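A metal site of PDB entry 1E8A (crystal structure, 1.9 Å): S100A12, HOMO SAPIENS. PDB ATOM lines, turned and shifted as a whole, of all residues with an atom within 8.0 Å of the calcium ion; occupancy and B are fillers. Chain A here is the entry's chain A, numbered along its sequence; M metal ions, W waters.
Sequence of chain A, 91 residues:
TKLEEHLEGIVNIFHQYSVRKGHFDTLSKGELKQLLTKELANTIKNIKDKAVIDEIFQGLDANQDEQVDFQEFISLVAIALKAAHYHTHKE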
ATOM      1  N   PHE A  14      10.884  19.577  20.875  1.00  0.00           N
ATOM      2  CA  PHE A  14       9.996  18.836  20.074  1.00  0.00           C
ATOM      3  C   PHE A  14       8.914  19.766  19.541  1.00  0.00           C
ATOM      4  O   PHE A  14       8.629  19.794  18.353  1.00  0.00           O
ATOM      5  CB  PHE A  14       9.374  17.662  20.851  1.00  0.00           C
ATOM      6  CG  PHE A  14       8.247  16.981  20.112  1.00  0.00           C
ATOM      7  CD1 PHE A  14       8.499  15.949  19.209  1.00  0.00           C
ATOM      8  CD2 PHE A  14       6.914  17.346  20.317  1.00  0.00           C
ATOM      9  CE1 PHE A  14       7.509  15.340  18.517  1.00  0.00           C
ATOM     10  CE2 PHE A  14       5.898  16.689  19.647  1.00  0.00           C
ATOM     11  CZ  PHE A  14       6.191  15.679  18.711  1.00  0.00           C
ATOM     12  N   HIS A  15       8.298  20.528  20.423  1.00  0.00           N
ATOM     13  CA  HIS A  15       7.262  21.430  19.977  1.00  0.00           C
ATOM     14  C   HIS A  15       7.801  22.627  19.187  1.00  0.00           C
ATOM     15  O   HIS A  15       7.106  23.162  18.307  1.00  0.00           O
ATOM     16  CB  HIS A  15       6.425  21.924  21.150  1.00  0.00           C
ATOM     17  CG  HIS A  15       5.503  20.879  21.678  1.00  0.00           C
ATOM     18  ND1 HIS A  15       5.786  20.198  22.842  1.00  0.00           N
ATOM     19  CD2 HIS A  15       4.543  20.152  21.067  1.00  0.00           C
ATOM     20  CE1 HIS A  15       4.849  19.274  23.029  1.00  0.00           C
ATOM     21  NE2 HIS A  15       4.018  19.311  22.014  1.00  0.00           N
ATOM     22  N   TYR A  17       9.621  22.566  16.858  1.00  0.00           N
ATOM     23  CA  TYR A  17       9.488  22.106  15.484  1.00  0.00           C
ATOM     24  C   TYR A  17       8.105  21.529  15.132  1.00  0.00           C
ATOM     25  O   TYR A  17       7.655  21.685  13.984  1.00  0.00           O
ATOM     26  CB  TYR A  17      10.618  21.156  15.136  1.00  0.00           C
ATOM     27  CG  TYR A  17      11.967  21.804  15.103  1.00  0.00           C
ATOM     28  CD1 TYR A  17      12.408  22.445  13.967  1.00  0.00           C
ATOM     29  CD2 TYR A  17      12.768  21.879  16.254  1.00  0.00           C
ATOM     30  CE1 TYR A  17      13.612  23.093  13.973  1.00  0.00           C
ATOM     31  CE2 TYR A  17      13.983  22.524  16.247  1.00  0.00           C
ATOM     32  CZ  TYR A  17      14.381  23.110  15.119  1.00  0.00           C
ATOM     33  OH  TYR A  17      15.563  23.767  15.117  1.00  0.00           O
ATOM     34  N   SER A  18       7.415  20.853  16.059  1.00  0.00           N
ATOM     35  CA  SER A  18       6.168  20.190  15.685  1.00  0.00           C
ATOM     36  C   SER A  18       5.000  21.140  15.376  1.00  0.00           C
ATOM     37  O   SER A  18       4.061  20.779  14.620  1.00  0.00           O
ATOM     38  CB  SER A  18       5.689  19.223  16.764  1.00  0.00           C
ATOM     39  OG  SER A  18       5.302  19.874  17.977  1.00  0.00           O
ATOM     40  N   VAL A  19       5.031  22.346  15.927  1.00  0.00           N
ATOM     41  CA  VAL A  19       3.945  23.240  15.706  1.00  0.00           C
ATOM     42  C   VAL A  19       4.020  23.940  14.377  1.00  0.00           C
ATOM     43  O   VAL A  19       3.107  24.660  13.997  1.00  0.00           O
ATOM     44  CB  VAL A  19       3.824  24.302  16.779  1.00  0.00           C
ATOM     45  CG1 VAL A  19       3.692  23.688  18.243  1.00  0.00           C
ATOM     46  CG2 VAL A  19       4.977  25.277  16.697  1.00  0.00           C
ATOM     47  N   ARG A  20       5.149  23.826  13.707  1.00  0.00           N
ATOM     48  CA  ARG A  20       5.364  24.654  12.526  1.00  0.00           C
ATOM     49  C   ARG A  20       4.425  24.370  11.334  1.00  0.00           C
ATOM     50  O   ARG A  20       3.996  25.321  10.634  1.00  0.00           O
ATOM     51  CB  ARG A  20       6.842  24.630  12.082  1.00  0.00           C
ATOM     52  CG  ARG A  20       7.867  25.049  13.128  1.00  0.00           C
ATOM     53  CD  ARG A  20       9.341  24.710  12.798  1.00  0.00           C
ATOM     54  NE  ARG A  20      10.242  25.364  13.703  1.00  0.00           N
ATOM     55  CZ  ARG A  20      11.441  25.771  13.395  1.00  0.00           C
ATOM     56  NH1 ARG A  20      11.925  25.558  12.181  1.00  0.00           N
ATOM     57  NH2 ARG A  20      12.175  26.371  14.326  1.00  0.00           N
ATOM     58  N   LYS A  21       4.141  23.126  11.042  1.00  0.00           N
ATOM     59  CA  LYS A  21       3.278  22.823   9.930  1.00  0.00           C
ATOM     60  C   LYS A  21       2.328  21.715  10.332  1.00  0.00           C
ATOM     61  O   LYS A  21       2.656  20.876  11.165  1.00  0.00           O
ATOM     62  CB  LYS A  21       4.141  22.397   8.712  1.00  0.00           C
ATOM     63  CG  LYS A  21       4.997  23.548   8.064  1.00  0.00           C
ATOM     64  CD  LYS A  21       4.274  24.318   7.013  1.00  0.00           C
ATOM     65  N   GLY A  22       1.126  21.695   9.772  1.00  0.00           N
ATOM     66  CA  GLY A  22       0.165  20.618  10.022  1.00  0.00           C
ATOM     67  C   GLY A  22      -0.143  20.436  11.484  1.00  0.00           C
ATOM     68  O   GLY A  22      -0.251  21.445  12.196  1.00  0.00           O
ATOM     69  N   HIS A  23      -0.366  19.203  11.908  1.00  0.00           N
ATOM     70  CA  HIS A  23      -0.683  18.908  13.320  1.00  0.00           C
ATOM     71  C   HIS A  23       0.363  19.514  14.275  1.00  0.00           C
ATOM     72  O   HIS A  23       1.557  19.362  14.028  1.00  0.00           O
ATOM     73  CB  HIS A  23      -0.805  17.385  13.566  1.00  0.00           C
ATOM     74  CG  HIS A  23      -1.409  17.030  14.888  1.00  0.00           C
ATOM     75  ND1 HIS A  23      -2.731  16.605  15.031  1.00  0.00           N
ATOM     76  CD2 HIS A  23      -0.901  17.093  16.144  1.00  0.00           C
ATOM     77  CE1 HIS A  23      -2.923  16.252  16.301  1.00  0.00           C
ATOM     78  NE2 HIS A  23      -1.871  16.635  17.005  1.00  0.00           N
ATOM     79  N   PHE A  24      -0.096  20.095  15.389  1.00  0.00           N
ATOM     80  CA  PHE A  24       0.770  20.731  16.372  1.00  0.00           C
ATOM     81  C   PHE A  24       1.606  19.764  17.188  1.00  0.00           C
ATOM     82  O   PHE A  24       2.609  20.168  17.746  1.00  0.00           O
ATOM     83  CB  PHE A  24      -0.009  21.621  17.371  1.00  0.00           C
ATOM     84  CG  PHE A  24      -0.439  22.961  16.820  1.00  0.00           C
ATOM     85  CD1 PHE A  24      -0.240  23.300  15.511  1.00  0.00           C
ATOM     86  CD2 PHE A  24      -0.962  23.942  17.670  1.00  0.00           C
ATOM     87  CE1 PHE A  24      -0.612  24.539  15.037  1.00  0.00           C
ATOM     88  CE2 PHE A  24      -1.339  25.157  17.175  1.00  0.00           C
ATOM     89  CZ  PHE A  24      -1.201  25.440  15.840  1.00  0.00           C
ATOM     90  N   ASP A  25       1.196  18.511  17.270  1.00  0.00           N
ATOM     91  CA  ASP A  25       1.817  17.552  18.202  1.00  0.00           C
ATOM     92  C   ASP A  25       2.514  16.421  17.466  1.00  0.00           C
ATOM     93  O   ASP A  25       2.823  15.397  18.054  1.00  0.00           O
ATOM     94  CB  ASP A  25       0.760  16.975  19.095  1.00  0.00           C
ATOM     95  CG  ASP A  25       1.305  16.439  20.472  1.00  0.00           C
ATOM     96  OD1 ASP A  25       2.345  16.887  20.997  1.00  0.00           O
ATOM     97  OD2 ASP A  25       0.691  15.563  21.128  1.00  0.00           O
ATOM     98  N   THR A  26       2.730  16.573  16.163  1.00  0.00           N
ATOM     99  CA  THR A  26       3.523  15.618  15.420  1.00  0.00           C
ATOM    100  C   THR A  26       4.447  16.329  14.440  1.00  0.00           C
ATOM    101  O   THR A  26       4.174  17.427  14.006  1.00  0.00           O
ATOM    102  CB  THR A  26       2.707  14.548  14.696  1.00  0.00           C
ATOM    103  OG1 THR A  26       1.997  15.118  13.601  1.00  0.00           O
ATOM    104  CG2 THR A  26       1.595  13.956  15.548  1.00  0.00           C
ATOM    105  N   LEU A  27       5.549  15.676  14.134  1.00  0.00           N
ATOM    106  CA  LEU A  27       6.581  16.171  13.215  1.00  0.00           C
ATOM    107  C   LEU A  27       6.373  15.593  11.852  1.00  0.00           C
ATOM    108  O   LEU A  27       6.360  14.367  11.663  1.00  0.00           O
ATOM    109  CB  LEU A  27       7.984  15.777  13.699  1.00  0.00           C
ATOM    110  CG  LEU A  27       8.401  16.321  15.054  1.00  0.00           C
ATOM    111  CD1 LEU A  27       9.576  15.521  15.582  1.00  0.00           C
ATOM    112  CD2 LEU A  27       8.790  17.776  14.983  1.00  0.00           C
ATOM    113  N   SER A  28       6.243  16.488  10.875  1.00  0.00           N
ATOM    114  CA  SER A  28       6.255  16.084   9.486  1.00  0.00           C
ATOM    115  C   SER A  28       7.683  15.783   9.049  1.00  0.00           C
ATOM    116  O   SER A  28       8.659  16.052   9.778  1.00  0.00           O
ATOM    117  CB  SER A  28       5.713  17.175   8.592  1.00  0.00           C
ATOM    118  OG  SER A  28       6.565  18.288   8.670  1.00  0.00           O
ATOM    119  N   LYS A  29       7.828  15.259   7.842  1.00  0.00           N
ATOM    120  CA  LYS A  29       9.164  14.899   7.398  1.00  0.00           C
ATOM    121  C   LYS A  29       9.982  16.194   7.348  1.00  0.00           C
ATOM    122  O   LYS A  29      11.114  16.236   7.752  1.00  0.00           O
ATOM    123  CB  LYS A  29       9.171  14.175   6.032  1.00  0.00           C
ATOM    124  N   GLU A  31       9.557  18.995   9.098  1.00  0.00           N
ATOM    125  CA  GLU A  31       9.823  19.476  10.431  1.00  0.00           C
ATOM    126  C   GLU A  31      10.950  18.661  11.049  1.00  0.00           C
ATOM    127  O   GLU A  31      11.872  19.241  11.650  1.00  0.00           O
ATOM    128  CB  GLU A  31       8.563  19.432  11.333  1.00  0.00           C
ATOM    129  CG  GLU A  31       7.454  20.393  10.921  1.00  0.00           C
ATOM    130  CD  GLU A  31       6.169  20.138  11.686  1.00  0.00           C
ATOM    131  OE1 GLU A  31       5.894  18.965  12.026  1.00  0.00           O
ATOM    132  OE2 GLU A  31       5.475  21.100  12.020  1.00  0.00           O
ATOM    133  N   LEU A  32      10.899  17.340  10.884  1.00  0.00           N
ATOM    134  CA  LEU A  32      11.969  16.502  11.402  1.00  0.00           C
ATOM    135  C   LEU A  32      13.293  16.842  10.741  1.00  0.00           C
ATOM    136  O   LEU A  32      14.312  16.924  11.411  1.00  0.00           O
ATOM    137  CB  LEU A  32      11.685  15.031  11.251  1.00  0.00           C
ATOM    138  CG  LEU A  32      12.760  14.099  11.860  1.00  0.00           C
ATOM    139  CD1 LEU A  32      12.812  14.198  13.368  1.00  0.00           C
ATOM    140  CD2 LEU A  32      12.552  12.708  11.429  1.00  0.00           C
ATOM    141  N   GLN A  67       4.187  10.897   9.876  1.00  0.00           N
ATOM    142  CA  GLN A  67       4.425  11.874  10.946  1.00  0.00           C
ATOM    143  C   GLN A  67       5.188  11.174  12.007  1.00  0.00           C
ATOM    144  O   GLN A  67       5.028   9.949  12.186  1.00  0.00           O
ATOM    145  CB  GLN A  67       3.125  12.261  11.598  1.00  0.00           C
ATOM    146  CG  GLN A  67       2.183  12.870  10.644  1.00  0.00           C
ATOM    147  CD  GLN A  67       2.593  14.285  10.316  1.00  0.00           C
ATOM    148  OE1 GLN A  67       3.036  15.022  11.211  1.00  0.00           O
ATOM    149  NE2 GLN A  67       2.441  14.681   9.076  1.00  0.00           N
ATOM    150  N   VAL A  68       6.011  11.928  12.724  1.00  0.00           N
ATOM    151  CA  VAL A  68       6.641  11.429  13.902  1.00  0.00           C
ATOM    152  C   VAL A  68       6.016  12.021  15.146  1.00  0.00           C
ATOM    153  O   VAL A  68       6.132  13.236  15.431  1.00  0.00           O
ATOM    154  CB  VAL A  68       8.175  11.604  13.842  1.00  0.00           C
ATOM    155  CG1 VAL A  68       8.779  11.135  15.141  1.00  0.00           C
ATOM    156  CG2 VAL A  68       8.794  10.852  12.604  1.00  0.00           C
HETATM  157 CA    CA M   1       3.658  19.438  12.784  1.00  0.00          CA
HETATM  158  O   HOH W   1       3.052  17.814  11.157  1.00  0.00           O
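OE2 of Glu 31 lies close to N of Arg 20 (3.2 Å).
OG of Ser 18 lies within hydrogen-bond range of O of Phe 14, at 3.3 Å.
The backbone NH of Glu 31 sits at hydrogen-bond distance from the side-chain hydroxyl of Ser 28 (3.1 Å).
OG of Ser 18 sits at hydrogen-bond distance from O of Phe 24, at 2.7 Å.
The side-chain hydroxyl (OG1) of Thr 26 is in hydrogen-bond range of the side-chain amide oxygen (OE1) of Gln 67, at 2.6 Å.
Five residues have an atom within 4 Å of the calcium ion: Ser 18, Lys 21, His 23, Thr 26 and Glu 31.
The calcium ion is bound by the backbone carbonyl oxygen (O) of Ser 18 (2.3 Å), water W1 (2.4 Å), the backbone carbonyl oxygen (O) of Lys 21 (2.4 Å), the side-chain carboxylate (OE1) of Glu 31 (2.4 Å), the backbone carbonyl oxygen (O) of Thr 26 (2.4 Å), the backbone carbonyl oxygen (O) of His 23 (2.4 Å) and the side-chain carboxylate (OE2) of Glu 31 (2.6 Å).
Water W1 lies within hydrogen-bond range of the side-chain amide oxygen (OE1) of Gln 67 (2.8 Å) and the backbone NH (N) of Ser 28 (3.5 Å).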
